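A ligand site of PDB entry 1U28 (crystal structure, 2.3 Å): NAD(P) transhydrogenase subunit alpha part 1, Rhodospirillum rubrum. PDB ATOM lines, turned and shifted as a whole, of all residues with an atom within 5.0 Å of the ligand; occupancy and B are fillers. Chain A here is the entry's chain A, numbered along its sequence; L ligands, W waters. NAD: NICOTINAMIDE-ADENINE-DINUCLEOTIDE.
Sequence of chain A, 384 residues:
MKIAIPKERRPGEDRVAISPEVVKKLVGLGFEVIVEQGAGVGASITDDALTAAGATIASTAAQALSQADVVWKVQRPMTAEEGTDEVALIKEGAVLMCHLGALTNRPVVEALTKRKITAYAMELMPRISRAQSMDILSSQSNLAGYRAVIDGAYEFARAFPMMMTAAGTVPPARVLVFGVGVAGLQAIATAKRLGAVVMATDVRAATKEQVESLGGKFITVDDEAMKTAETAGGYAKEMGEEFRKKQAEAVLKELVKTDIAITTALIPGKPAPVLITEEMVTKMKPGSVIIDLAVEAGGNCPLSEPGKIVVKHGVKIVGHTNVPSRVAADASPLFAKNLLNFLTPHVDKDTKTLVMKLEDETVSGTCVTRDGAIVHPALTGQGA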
ATOM      1  N   PRO A 126     -17.163  19.489 -19.511  1.00  0.00           N
ATOM      2  CA  PRO A 126     -18.454  19.492 -18.822  1.00  0.00           C
ATOM      3  C   PRO A 126     -18.525  18.581 -17.601  1.00  0.00           C
ATOM      4  O   PRO A 126     -17.917  17.506 -17.599  1.00  0.00           O
ATOM      5  CB  PRO A 126     -19.419  19.010 -19.907  1.00  0.00           C
ATOM      6  CG  PRO A 126     -18.841  19.506 -21.162  1.00  0.00           C
ATOM      7  CD  PRO A 126     -17.344  19.406 -20.981  1.00  0.00           C
ATOM      8  N   ARG A 127     -19.262  19.005 -16.585  1.00  0.00           N
ATOM      9  CA  ARG A 127     -19.402  18.255 -15.342  1.00  0.00           C
ATOM     10  C   ARG A 127     -20.577  17.277 -15.417  1.00  0.00           C
ATOM     11  O   ARG A 127     -21.338  17.136 -14.451  1.00  0.00           O
ATOM     12  CB  ARG A 127     -19.601  19.226 -14.167  1.00  0.00           C
ATOM     13  CG  ARG A 127     -18.518  20.292 -14.029  1.00  0.00           C
ATOM     14  CD  ARG A 127     -17.206  19.714 -13.527  1.00  0.00           C
ATOM     15  NE  ARG A 127     -16.982  19.985 -12.097  1.00  0.00           N
ATOM     16  CZ  ARG A 127     -16.031  20.771 -11.596  1.00  0.00           C
ATOM     17  NH1 ARG A 127     -15.165  21.412 -12.385  1.00  0.00           N
ATOM     18  NH2 ARG A 127     -15.928  20.931 -10.276  1.00  0.00           N
ATOM     19  N   ILE A 128     -20.700  16.589 -16.558  1.00  0.00           N
ATOM     20  CA  ILE A 128     -21.742  15.565 -16.749  1.00  0.00           C
ATOM     21  C   ILE A 128     -21.110  14.175 -16.632  1.00  0.00           C
ATOM     22  O   ILE A 128     -19.947  13.985 -16.964  1.00  0.00           O
ATOM     23  CB  ILE A 128     -22.458  15.722 -18.115  1.00  0.00           C
ATOM     24  CG1 ILE A 128     -21.461  15.922 -19.264  1.00  0.00           C
ATOM     25  CG2 ILE A 128     -23.442  16.901 -18.068  1.00  0.00           C
ATOM     26  CD1 ILE A 128     -22.028  15.628 -20.636  1.00  0.00           C
ATOM     27  N   SER A 129     -21.895  13.213 -16.141  1.00  0.00           N
ATOM     28  CA  SER A 129     -21.355  11.913 -15.694  1.00  0.00           C
ATOM     29  C   SER A 129     -20.615  11.116 -16.773  1.00  0.00           C
ATOM     30  O   SER A 129     -19.662  10.408 -16.472  1.00  0.00           O
ATOM     31  CB  SER A 129     -22.479  11.036 -15.112  1.00  0.00           C
ATOM     32  OG  SER A 129     -21.932   9.923 -14.412  1.00  0.00           O
ATOM     33  N   ALA A 131     -18.727  12.152 -19.156  1.00  0.00           N
ATOM     34  CA  ALA A 131     -17.426  12.718 -19.478  1.00  0.00           C
ATOM     35  C   ALA A 131     -16.336  12.402 -18.440  1.00  0.00           C
ATOM     36  O   ALA A 131     -15.202  12.818 -18.614  1.00  0.00           O
ATOM     37  CB  ALA A 131     -17.548  14.219 -19.667  1.00  0.00           C
ATOM     38  N   GLN A 132     -16.675  11.675 -17.375  1.00  0.00           N
ATOM     39  CA  GLN A 132     -15.714  11.260 -16.347  1.00  0.00           C
ATOM     40  C   GLN A 132     -14.482  10.490 -16.888  1.00  0.00           C
ATOM     41  O   GLN A 132     -13.390  10.593 -16.330  1.00  0.00           O
ATOM     42  CB  GLN A 132     -16.403  10.435 -15.240  1.00  0.00           C
ATOM     43  CG  GLN A 132     -17.088  11.277 -14.162  1.00  0.00           C
ATOM     44  CD  GLN A 132     -18.123  10.495 -13.329  1.00  0.00           C
ATOM     45  OE1 GLN A 132     -17.922  10.244 -12.132  1.00  0.00           O
ATOM     46  NE2 GLN A 132     -19.224  10.111 -13.958  1.00  0.00           N
ATOM     47  N   ASP A 135     -12.143  13.180 -18.297  1.00  0.00           N
ATOM     48  CA  ASP A 135     -12.043  14.273 -17.328  1.00  0.00           C
ATOM     49  C   ASP A 135     -10.669  14.274 -16.639  1.00  0.00           C
ATOM     50  O   ASP A 135     -10.357  13.395 -15.842  1.00  0.00           O
ATOM     51  CB  ASP A 135     -13.166  14.086 -16.313  1.00  0.00           C
ATOM     52  CG  ASP A 135     -13.246  15.185 -15.278  1.00  0.00           C
ATOM     53  OD1 ASP A 135     -13.876  14.914 -14.228  1.00  0.00           O
ATOM     54  OD2 ASP A 135     -12.707  16.295 -15.484  1.00  0.00           O
ATOM     55  N   SER A 138     -10.297  15.123 -12.523  1.00  0.00           N
ATOM     56  CA  SER A 138     -10.559  13.959 -11.682  1.00  0.00           C
ATOM     57  C   SER A 138      -9.442  12.933 -11.667  1.00  0.00           C
ATOM     58  O   SER A 138      -9.101  12.409 -10.604  1.00  0.00           O
ATOM     59  CB  SER A 138     -11.848  13.253 -12.153  1.00  0.00           C
ATOM     60  OG  SER A 138     -12.991  14.045 -11.922  1.00  0.00           O
ATOM     61  N   SER A 141      -6.351  14.884  -9.930  1.00  0.00           N
ATOM     62  CA  SER A 141      -6.566  15.298  -8.539  1.00  0.00           C
ATOM     63  C   SER A 141      -6.736  14.110  -7.577  1.00  0.00           C
ATOM     64  O   SER A 141      -6.397  14.207  -6.396  1.00  0.00           O
ATOM     65  CB  SER A 141      -7.759  16.238  -8.425  1.00  0.00           C
ATOM     66  OG  SER A 141      -8.939  15.539  -8.697  1.00  0.00           O
ATOM     67  N   PHE A 178      -9.728  19.057   4.717  1.00  0.00           N
ATOM     68  CA  PHE A 178     -10.608  20.189   4.428  1.00  0.00           C
ATOM     69  C   PHE A 178     -10.963  20.171   2.952  1.00  0.00           C
ATOM     70  O   PHE A 178     -10.121  20.490   2.108  1.00  0.00           O
ATOM     71  CB  PHE A 178      -9.911  21.521   4.707  1.00  0.00           C
ATOM     72  CG  PHE A 178      -9.631  21.784   6.157  1.00  0.00           C
ATOM     73  CD1 PHE A 178     -10.338  22.759   6.847  1.00  0.00           C
ATOM     74  CD2 PHE A 178      -8.635  21.085   6.832  1.00  0.00           C
ATOM     75  CE1 PHE A 178     -10.086  23.026   8.179  1.00  0.00           C
ATOM     76  CE2 PHE A 178      -8.362  21.347   8.168  1.00  0.00           C
ATOM     77  CZ  PHE A 178      -9.102  22.325   8.843  1.00  0.00           C
ATOM     78  N   GLY A 179     -12.201  19.808   2.639  1.00  0.00           N
ATOM     79  CA  GLY A 179     -12.640  19.682   1.253  1.00  0.00           C
ATOM     80  C   GLY A 179     -12.568  18.219   0.832  1.00  0.00           C
ATOM     81  O   GLY A 179     -11.479  17.614   0.866  1.00  0.00           O
ATOM     82  N   VAL A 180     -13.720  17.678   0.441  1.00  0.00           N
ATOM     83  CA  VAL A 180     -13.880  16.271   0.130  1.00  0.00           C
ATOM     84  C   VAL A 180     -14.442  16.106  -1.286  1.00  0.00           C
ATOM     85  O   VAL A 180     -15.500  15.516  -1.500  1.00  0.00           O
ATOM     86  CB  VAL A 180     -14.797  15.583   1.167  1.00  0.00           C
ATOM     87  CG1 VAL A 180     -14.778  14.061   1.006  1.00  0.00           C
ATOM     88  CG2 VAL A 180     -14.370  15.953   2.587  1.00  0.00           C
ATOM     89  N   GLY A 181     -13.725  16.668  -2.267  1.00  0.00           N
ATOM     90  CA  GLY A 181     -13.944  16.366  -3.669  1.00  0.00           C
ATOM     91  C   GLY A 181     -13.123  15.142  -4.029  1.00  0.00           C
ATOM     92  O   GLY A 181     -12.894  14.261  -3.192  1.00  0.00           O
ATOM     93  N   VAL A 182     -12.643  15.091  -5.267  1.00  0.00           N
ATOM     94  CA  VAL A 182     -11.921  13.924  -5.764  1.00  0.00           C
ATOM     95  C   VAL A 182     -10.601  13.693  -4.998  1.00  0.00           C
ATOM     96  O   VAL A 182     -10.300  12.570  -4.598  1.00  0.00           O
ATOM     97  CB  VAL A 182     -11.682  14.008  -7.298  1.00  0.00           C
ATOM     98  CG1 VAL A 182     -10.881  12.823  -7.792  1.00  0.00           C
ATOM     99  CG2 VAL A 182     -13.018  14.078  -8.037  1.00  0.00           C
ATOM    100  N   ALA A 183      -9.842  14.775  -4.796  1.00  0.00           N
ATOM    101  CA  ALA A 183      -8.581  14.734  -4.043  1.00  0.00           C
ATOM    102  C   ALA A 183      -8.771  14.396  -2.557  1.00  0.00           C
ATOM    103  O   ALA A 183      -8.018  13.589  -1.988  1.00  0.00           O
ATOM    104  CB  ALA A 183      -7.812  16.057  -4.194  1.00  0.00           C
ATOM    105  N   THR A 201     -14.259  17.670   6.501  1.00  0.00           N
ATOM    106  CA  THR A 201     -15.301  18.687   6.355  1.00  0.00           C
ATOM    107  C   THR A 201     -15.384  19.182   4.913  1.00  0.00           C
ATOM    108  O   THR A 201     -14.412  19.128   4.168  1.00  0.00           O
ATOM    109  CB  THR A 201     -15.093  19.883   7.319  1.00  0.00           C
ATOM    110  OG1 THR A 201     -16.287  20.683   7.346  1.00  0.00           O
ATOM    111  CG2 THR A 201     -13.897  20.745   6.905  1.00  0.00           C
ATOM    112  N   ASP A 202     -16.573  19.654   4.551  1.00  0.00           N
ATOM    113  CA  ASP A 202     -16.868  20.216   3.231  1.00  0.00           C
ATOM    114  C   ASP A 202     -18.151  21.036   3.375  1.00  0.00           C
ATOM    115  O   ASP A 202     -18.925  20.822   4.302  1.00  0.00           O
ATOM    116  CB  ASP A 202     -17.067  19.089   2.213  1.00  0.00           C
ATOM    117  CG  ASP A 202     -17.014  19.582   0.771  1.00  0.00           C
ATOM    118  OD1 ASP A 202     -17.804  20.476   0.396  1.00  0.00           O
ATOM    119  OD2 ASP A 202     -16.195  19.056   0.001  1.00  0.00           O
ATOM    120  N   VAL A 203     -18.352  21.983   2.458  1.00  0.00           N
ATOM    121  CA  VAL A 203     -19.573  22.805   2.456  1.00  0.00           C
ATOM    122  C   VAL A 203     -20.781  22.084   1.814  1.00  0.00           C
ATOM    123  O   VAL A 203     -21.918  22.425   2.101  1.00  0.00           O
ATOM    124  CB  VAL A 203     -19.344  24.187   1.775  1.00  0.00           C
ATOM    125  CG1 VAL A 203     -18.316  24.986   2.551  1.00  0.00           C
ATOM    126  CG2 VAL A 203     -18.922  24.039   0.311  1.00  0.00           C
ATOM    127  N   ARG A 204     -20.523  21.090   0.960  1.00  0.00           N
ATOM    128  CA  ARG A 204     -21.581  20.351   0.271  1.00  0.00           C
ATOM    129  C   ARG A 204     -22.118  19.195   1.132  1.00  0.00           C
ATOM    130  O   ARG A 204     -21.348  18.397   1.671  1.00  0.00           O
ATOM    131  CB  ARG A 204     -21.081  19.826  -1.069  1.00  0.00           C
ATOM    132  CG  ARG A 204     -20.491  20.904  -1.970  1.00  0.00           C
ATOM    133  CD  ARG A 204     -20.148  20.385  -3.365  1.00  0.00           C
ATOM    134  NE  ARG A 204     -18.977  19.512  -3.392  1.00  0.00           N
ATOM    135  CZ  ARG A 204     -18.987  18.183  -3.254  1.00  0.00           C
ATOM    136  NH1 ARG A 204     -20.130  17.517  -3.065  1.00  0.00           N
ATOM    137  NH2 ARG A 204     -17.847  17.500  -3.301  1.00  0.00           N
ATOM    138  N   THR A 207     -21.282  15.182   0.954  1.00  0.00           N
ATOM    139  CA  THR A 207     -19.965  14.732   1.412  1.00  0.00           C
ATOM    140  C   THR A 207     -20.032  13.889   2.683  1.00  0.00           C
ATOM    141  O   THR A 207     -19.209  12.980   2.870  1.00  0.00           O
ATOM    142  CB  THR A 207     -19.065  15.945   1.671  1.00  0.00           C
ATOM    143  OG1 THR A 207     -18.668  16.499   0.410  1.00  0.00           O
ATOM    144  CG2 THR A 207     -17.830  15.549   2.457  1.00  0.00           C
ATOM    145  N   GLU A 230     -23.934  23.202  -2.590  1.00  0.00           N
ATOM    146  CA  GLU A 230     -23.627  22.599  -3.891  1.00  0.00           C
ATOM    147  C   GLU A 230     -24.494  23.237  -4.979  1.00  0.00           C
ATOM    148  O   GLU A 230     -25.655  23.598  -4.730  1.00  0.00           O
ATOM    149  CB  GLU A 230     -23.833  21.077  -3.858  1.00  0.00           C
ATOM    150  CG  GLU A 230     -23.394  20.355  -5.128  1.00  0.00           C
ATOM    151  CD  GLU A 230     -23.230  18.842  -4.972  1.00  0.00           C
ATOM    152  OE1 GLU A 230     -23.314  18.333  -3.829  1.00  0.00           O
ATOM    153  OE2 GLU A 230     -23.012  18.161  -5.994  1.00  0.00           O
ATOM    154  N   GLY A 233     -23.633  22.618 -11.131  1.00  0.00           N
ATOM    155  CA  GLY A 233     -22.363  22.101 -11.643  1.00  0.00           C
ATOM    156  C   GLY A 233     -21.673  21.099 -10.728  1.00  0.00           C
ATOM    157  O   GLY A 233     -20.810  20.335 -11.179  1.00  0.00           O
ATOM    158  N   GLY A 234     -22.028  21.106  -9.443  1.00  0.00           N
ATOM    159  CA  GLY A 234     -21.425  20.201  -8.456  1.00  0.00           C
ATOM    160  C   GLY A 234     -20.246  20.806  -7.703  1.00  0.00           C
ATOM    161  O   GLY A 234     -19.680  20.161  -6.822  1.00  0.00           O
ATOM    162  N   TYR A 235     -19.894  22.039  -8.062  1.00  0.00           N
ATOM    163  CA  TYR A 235     -18.796  22.755  -7.393  1.00  0.00           C
ATOM    164  C   TYR A 235     -19.349  23.705  -6.336  1.00  0.00           C
ATOM    165  O   TYR A 235     -20.544  24.003  -6.296  1.00  0.00           O
ATOM    166  CB  TYR A 235     -17.893  23.498  -8.402  1.00  0.00           C
ATOM    167  CG  TYR A 235     -18.596  24.059  -9.616  1.00  0.00           C
ATOM    168  CD1 TYR A 235     -19.614  25.016  -9.480  1.00  0.00           C
ATOM    169  CD2 TYR A 235     -18.240  23.670 -10.899  1.00  0.00           C
ATOM    170  CE1 TYR A 235     -20.270  25.540 -10.598  1.00  0.00           C
ATOM    171  CE2 TYR A 235     -18.880  24.193 -12.025  1.00  0.00           C
ATOM    172  CZ  TYR A 235     -19.900  25.127 -11.865  1.00  0.00           C
ATOM    173  OH  TYR A 235     -20.545  25.655 -12.961  1.00  0.00           O
ATOM    174  N   ALA A 236     -18.464  24.166  -5.455  1.00  0.00           N
ATOM    175  CA  ALA A 236     -18.833  25.033  -4.346  1.00  0.00           C
ATOM    176  C   ALA A 236     -18.921  26.502  -4.781  1.00  0.00           C
ATOM    177  O   ALA A 236     -18.392  26.879  -5.825  1.00  0.00           O
ATOM    178  CB  ALA A 236     -17.823  24.890  -3.218  1.00  0.00           C
ATOM    179  N   MET A 239     -19.077  31.079   0.404  1.00  0.00           N
ATOM    180  CA  MET A 239     -20.038  30.884   1.496  1.00  0.00           C
ATOM    181  C   MET A 239     -20.281  32.134   2.334  1.00  0.00           C
ATOM    182  O   MET A 239     -21.393  32.355   2.812  1.00  0.00           O
ATOM    183  CB  MET A 239     -19.571  29.747   2.425  1.00  0.00           C
ATOM    184  CG  MET A 239     -19.540  28.377   1.785  1.00  0.00           C
ATOM    185  SD  MET A 239     -21.164  27.799   1.251  1.00  0.00           S
ATOM    186  CE  MET A 239     -22.029  27.597   2.811  1.00  0.00           C
ATOM    187  N   PHE A 243     -20.124  32.431   7.799  1.00  0.00           N
ATOM    188  CA  PHE A 243     -20.031  30.973   7.811  1.00  0.00           C
ATOM    189  C   PHE A 243     -18.596  30.556   8.116  1.00  0.00           C
ATOM    190  O   PHE A 243     -18.355  29.691   8.962  1.00  0.00           O
ATOM    191  CB  PHE A 243     -20.468  30.386   6.462  1.00  0.00           C
ATOM    192  CG  PHE A 243     -20.065  28.944   6.279  1.00  0.00           C
ATOM    193  CD1 PHE A 243     -20.908  27.922   6.691  1.00  0.00           C
ATOM    194  CD2 PHE A 243     -18.836  28.613   5.726  1.00  0.00           C
ATOM    195  CE1 PHE A 243     -20.529  26.586   6.536  1.00  0.00           C
ATOM    196  CE2 PHE A 243     -18.450  27.284   5.570  1.00  0.00           C
ATOM    197  CZ  PHE A 243     -19.301  26.268   5.981  1.00  0.00           C
ATOM    198  N   GLN A 247     -17.574  27.964  10.767  1.00  0.00           N
ATOM    199  CA  GLN A 247     -16.734  26.830  10.383  1.00  0.00           C
ATOM    200  C   GLN A 247     -15.438  26.747  11.211  1.00  0.00           C
ATOM    201  O   GLN A 247     -15.063  25.682  11.672  1.00  0.00           O
ATOM    202  CB  GLN A 247     -16.399  26.910   8.884  1.00  0.00           C
ATOM    203  CG  GLN A 247     -15.587  25.739   8.349  1.00  0.00           C
ATOM    204  CD  GLN A 247     -15.203  25.885   6.885  1.00  0.00           C
ATOM    205  OE1 GLN A 247     -15.463  25.002   6.060  1.00  0.00           O
ATOM    206  NE2 GLN A 247     -14.576  27.016   6.545  1.00  0.00           N
ATOM    207  N   THR A 264      -7.873  21.031   0.415  1.00  0.00           N
ATOM    208  CA  THR A 264      -8.062  20.780  -1.024  1.00  0.00           C
ATOM    209  C   THR A 264      -9.180  21.622  -1.652  1.00  0.00           C
ATOM    210  O   THR A 264      -9.580  21.365  -2.791  1.00  0.00           O
ATOM    211  CB  THR A 264      -8.391  19.272  -1.310  1.00  0.00           C
ATOM    212  OG1 THR A 264      -9.756  18.996  -0.969  1.00  0.00           O
ATOM    213  CG2 THR A 264      -7.482  18.333  -0.519  1.00  0.00           C
ATOM    214  N   ALA A 265      -9.650  22.639  -0.935  1.00  0.00           N
ATOM    215  CA  ALA A 265     -10.881  23.341  -1.296  1.00  0.00           C
ATOM    216  C   ALA A 265     -10.656  24.346  -2.430  1.00  0.00           C
ATOM    217  O   ALA A 265      -9.786  25.224  -2.329  1.00  0.00           O
ATOM    218  CB  ALA A 265     -11.480  24.016  -0.091  1.00  0.00           C
ATOM    219  N   LEU A 266     -11.459  24.193  -3.482  1.00  0.00           N
ATOM    220  CA  LEU A 266     -11.389  25.052  -4.673  1.00  0.00           C
ATOM    221  C   LEU A 266     -12.754  25.661  -5.004  1.00  0.00           C
ATOM    222  O   LEU A 266     -13.786  25.063  -4.709  1.00  0.00           O
ATOM    223  CB  LEU A 266     -10.884  24.221  -5.852  1.00  0.00           C
ATOM    224  CG  LEU A 266      -9.435  24.385  -6.302  1.00  0.00           C
ATOM    225  CD1 LEU A 266      -8.477  24.564  -5.141  1.00  0.00           C
ATOM    226  CD2 LEU A 266      -9.042  23.198  -7.173  1.00  0.00           C
ATOM    227  N   ILE A 267     -12.749  26.860  -5.590  1.00  0.00           N
ATOM    228  CA  ILE A 267     -13.960  27.522  -6.084  1.00  0.00           C
ATOM    229  C   ILE A 267     -13.686  28.071  -7.496  1.00  0.00           C
ATOM    230  O   ILE A 267     -12.894  29.007  -7.642  1.00  0.00           O
ATOM    231  CB  ILE A 267     -14.444  28.686  -5.161  1.00  0.00           C
ATOM    232  CG1 ILE A 267     -14.734  28.166  -3.747  1.00  0.00           C
ATOM    233  CG2 ILE A 267     -15.716  29.334  -5.723  1.00  0.00           C
ATOM    234  CD1 ILE A 267     -14.907  29.241  -2.712  1.00  0.00           C
ATOM    235  N   PRO A 268     -14.316  27.503  -8.526  1.00  0.00           N
ATOM    236  CA  PRO A 268     -14.108  27.924  -9.923  1.00  0.00           C
ATOM    237  C   PRO A 268     -14.158  29.437 -10.175  1.00  0.00           C
ATOM    238  O   PRO A 268     -15.097  30.119  -9.761  1.00  0.00           O
ATOM    239  CB  PRO A 268     -15.256  27.237 -10.655  1.00  0.00           C
ATOM    240  CG  PRO A 268     -15.437  25.966  -9.896  1.00  0.00           C
ATOM    241  CD  PRO A 268     -15.265  26.367  -8.457  1.00  0.00           C
ATOM    242  N   PRO A 273     -10.587  29.344  -0.942  1.00  0.00           N
ATOM    243  CA  PRO A 273     -11.113  29.807   0.344  1.00  0.00           C
ATOM    244  C   PRO A 273     -10.140  29.537   1.490  1.00  0.00           C
ATOM    245  O   PRO A 273      -9.479  28.496   1.504  1.00  0.00           O
ATOM    246  CB  PRO A 273     -12.394  28.983   0.523  1.00  0.00           C
ATOM    247  CG  PRO A 273     -12.163  27.745  -0.289  1.00  0.00           C
ATOM    248  CD  PRO A 273     -11.336  28.181  -1.456  1.00  0.00           C
ATOM    249  N   LEU A 275      -9.207  28.392   4.965  1.00  0.00           N
ATOM    250  CA  LEU A 275      -9.762  27.437   5.930  1.00  0.00           C
ATOM    251  C   LEU A 275      -8.955  27.355   7.222  1.00  0.00           C
ATOM    252  O   LEU A 275      -9.518  27.049   8.269  1.00  0.00           O
ATOM    253  CB  LEU A 275      -9.873  26.048   5.293  1.00  0.00           C
ATOM    254  CG  LEU A 275     -10.513  26.065   3.904  1.00  0.00           C
ATOM    255  CD1 LEU A 275     -10.613  24.670   3.342  1.00  0.00           C
ATOM    256  CD2 LEU A 275     -11.905  26.746   3.905  1.00  0.00           C
HETATM  257  PA  NAD L   1     -13.085  20.971  -6.270  1.00  0.00           P
HETATM  258  O1A NAD L   1     -11.702  20.628  -6.685  1.00  0.00           O
HETATM  259  O2A NAD L   1     -13.661  22.063  -7.114  1.00  0.00           O
HETATM  260  O5B NAD L   1     -13.092  21.368  -4.712  1.00  0.00           O
HETATM  261  C5B NAD L   1     -12.772  20.410  -3.724  1.00  0.00           C
HETATM  262  C4B NAD L   1     -13.780  20.424  -2.586  1.00  0.00           C
HETATM  263  O4B NAD L   1     -13.627  21.581  -1.776  1.00  0.00           O
HETATM  264  C3B NAD L   1     -15.236  20.431  -3.032  1.00  0.00           C
HETATM  265  O3B NAD L   1     -15.848  19.254  -2.567  1.00  0.00           O
HETATM  266  C2B NAD L   1     -15.848  21.694  -2.433  1.00  0.00           C
HETATM  267  O2B NAD L   1     -17.190  21.566  -2.005  1.00  0.00           O
HETATM  268  C1B NAD L   1     -14.900  21.938  -1.275  1.00  0.00           C
HETATM  269  N9A NAD L   1     -14.947  23.318  -0.731  1.00  0.00           N
HETATM  270  C8A NAD L   1     -15.014  24.494  -1.416  1.00  0.00           C
HETATM  271  N7A NAD L   1     -15.042  25.510  -0.523  1.00  0.00           N
HETATM  272  C5A NAD L   1     -14.989  24.990   0.724  1.00  0.00           C
HETATM  273  C6A NAD L   1     -14.998  25.575   1.989  1.00  0.00           C
HETATM  274  N6A NAD L   1     -15.509  26.800   2.115  1.00  0.00           N
HETATM  275  N1A NAD L   1     -14.926  24.759   3.120  1.00  0.00           N
HETATM  276  C2A NAD L   1     -14.875  23.385   2.976  1.00  0.00           C
HETATM  277  N3A NAD L   1     -14.875  22.823   1.716  1.00  0.00           N
HETATM  278  C4A NAD L   1     -14.940  23.606   0.602  1.00  0.00           C
HETATM  279  O3  NAD L   1     -14.060  19.676  -6.307  1.00  0.00           O
HETATM  280  PN  NAD L   1     -13.921  18.455  -7.351  1.00  0.00           P
HETATM  281  O1N NAD L   1     -12.826  17.570  -6.904  1.00  0.00           O
HETATM  282  O2N NAD L   1     -13.848  19.016  -8.701  1.00  0.00           O
HETATM  283  O5D NAD L   1     -15.297  17.664  -7.172  1.00  0.00           O
HETATM  284  C5D NAD L   1     -16.476  18.285  -6.697  1.00  0.00           C
HETATM  285  C4D NAD L   1     -17.705  17.486  -7.143  1.00  0.00           C
HETATM  286  O4D NAD L   1     -17.850  17.619  -8.545  1.00  0.00           O
HETATM  287  C3D NAD L   1     -17.596  15.989  -6.854  1.00  0.00           C
HETATM  288  O3D NAD L   1     -18.846  15.491  -6.414  1.00  0.00           O
HETATM  289  C2D NAD L   1     -17.235  15.388  -8.189  1.00  0.00           C
HETATM  290  O2D NAD L   1     -17.700  14.064  -8.395  1.00  0.00           O
HETATM  291  C1D NAD L   1     -17.952  16.332  -9.138  1.00  0.00           C
HETATM  292  N1N NAD L   1     -17.376  16.281 -10.506  1.00  0.00           N
HETATM  293  C2N NAD L   1     -18.157  15.916 -11.576  1.00  0.00           C
HETATM  294  C3N NAD L   1     -17.614  15.859 -12.854  1.00  0.00           C
HETATM  295  C7N NAD L   1     -18.400  15.199 -13.962  1.00  0.00           C
HETATM  296  O7N NAD L   1     -19.735  14.781 -13.724  1.00  0.00           O
HETATM  297  N7N NAD L   1     -17.831  15.014 -15.161  1.00  0.00           N
HETATM  298  C4N NAD L   1     -16.266  16.200 -13.045  1.00  0.00           C
HETATM  299  C5N NAD L   1     -15.489  16.556 -11.943  1.00  0.00           C
HETATM  300  C6N NAD L   1     -16.059  16.610 -10.678  1.00  0.00           C
HETATM  301  O   HOH W   1     -10.619  17.578  -5.326  1.00  0.00           O
HETATM  302  O   HOH W   2     -16.809  27.747  -0.491  1.00  0.00           O
HETATM  303  O   HOH W   3     -11.165  16.888  -9.446  1.00  0.00           O
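O of Ile 128 is in hydrogen-bond range of N7N of the ligand.
N of Gly 181 lies within hydrogen-bond range of O3B of the ligand (3.4 Å).
O7N of the ligand lies close to N of Ile 128 (3.5 Å).
The backbone carbonyl oxygen of Pro 126 sits at hydrogen-bond distance from a nitrogen (N7N) of the ligand.
O2N of the ligand lies within salt-bridge range of NH2 of Arg 127 (3.2 Å).
An oxygen (O1N) of the ligand sits at hydrogen-bond distance from the backbone NH (N) of Val 182 (3.0 Å).
The backbone NH of Leu 266 sits at hydrogen-bond distance from an oxygen (O5B) of the ligand (3.5 Å).
N1A of the ligand lies close to OE1 of Gln 247, 3.0 Å away.
The side-chain carboxylate of Asp 202 is in hydrogen-bond range of an oxygen (O3B) of the ligand (2.6 Å).
NH2 of Arg 204 sits at hydrogen-bond distance from O3B of the ligand, 2.8 Å away.
The side-chain carboxylate (OE1) of Glu 230 is in salt-bridge range of the guanidinium group (NH1) of Arg 204.
The side-chain hydroxyl of Thr 264 sits at hydrogen-bond distance from the backbone carbonyl oxygen of Gly 179.
OD1 of Asp 135 lies within hydrogen-bond range of OG of Ser 138 (2.6 Å).
OD2 of Asp 202 is in hydrogen-bond range of N of Val 180 (2.9 Å).
The backbone NH (N) of Arg 204 lies within hydrogen-bond range of the side-chain carboxylate (OD1) of Asp 202 (2.8 Å).
The backbone carbonyl oxygen (O) of Thr 201 lies within hydrogen-bond range of the backbone NH (N) of Gly 179.
The backbone carbonyl oxygen (O) of Phe 178 sits at hydrogen-bond distance from the backbone NH (N) of Thr 264 (2.9 Å).
The backbone carbonyl oxygen of Ser 129 lies within hydrogen-bond range of the side-chain amide nitrogen of Gln 132, 2.6 Å away.
Ser 129 touches the ligand.
Gln 132 touches the ligand (CG to N7N, 3.9 Å).
Asp 135 touches the ligand.
Ser 138 touches the ligand.
Gly 179 touches the ligand.
C of Val 180 touches O3B of the ligand (3.7 Å).
Val 203 touches the ligand (CG1 to N6A, 3.4 Å).
Gly 234 touches the ligand (O to C4D, 3.3 Å).
Ala 236 touches the ligand (CB to C8A, 3.4 Å).
Thr 264 touches the ligand (O to C5B, 3.5 Å).
CA of Ala 265 touches O4B of the ligand, at 3.3 Å.
Pro 273 touches the ligand (CG to N7A, 3.7 Å).
Leu 275 touches the ligand (CD2 to N1A, 3.7 Å).
The nearest printed residue that does not touch the ligand is Ile 267 (4.2 Å).
Water W1 lies within hydrogen-bond range of an oxygen (O1N) of the ligand (2.7 Å), the backbone NH of Ala 183 (3.0 Å) and the backbone NH of Val 182 (3.2 Å).
Water W3 bridges the side-chain hydroxyl of Ser 141 (2.7 Å) and an oxygen (O1N) of the ligand (3.1 Å).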
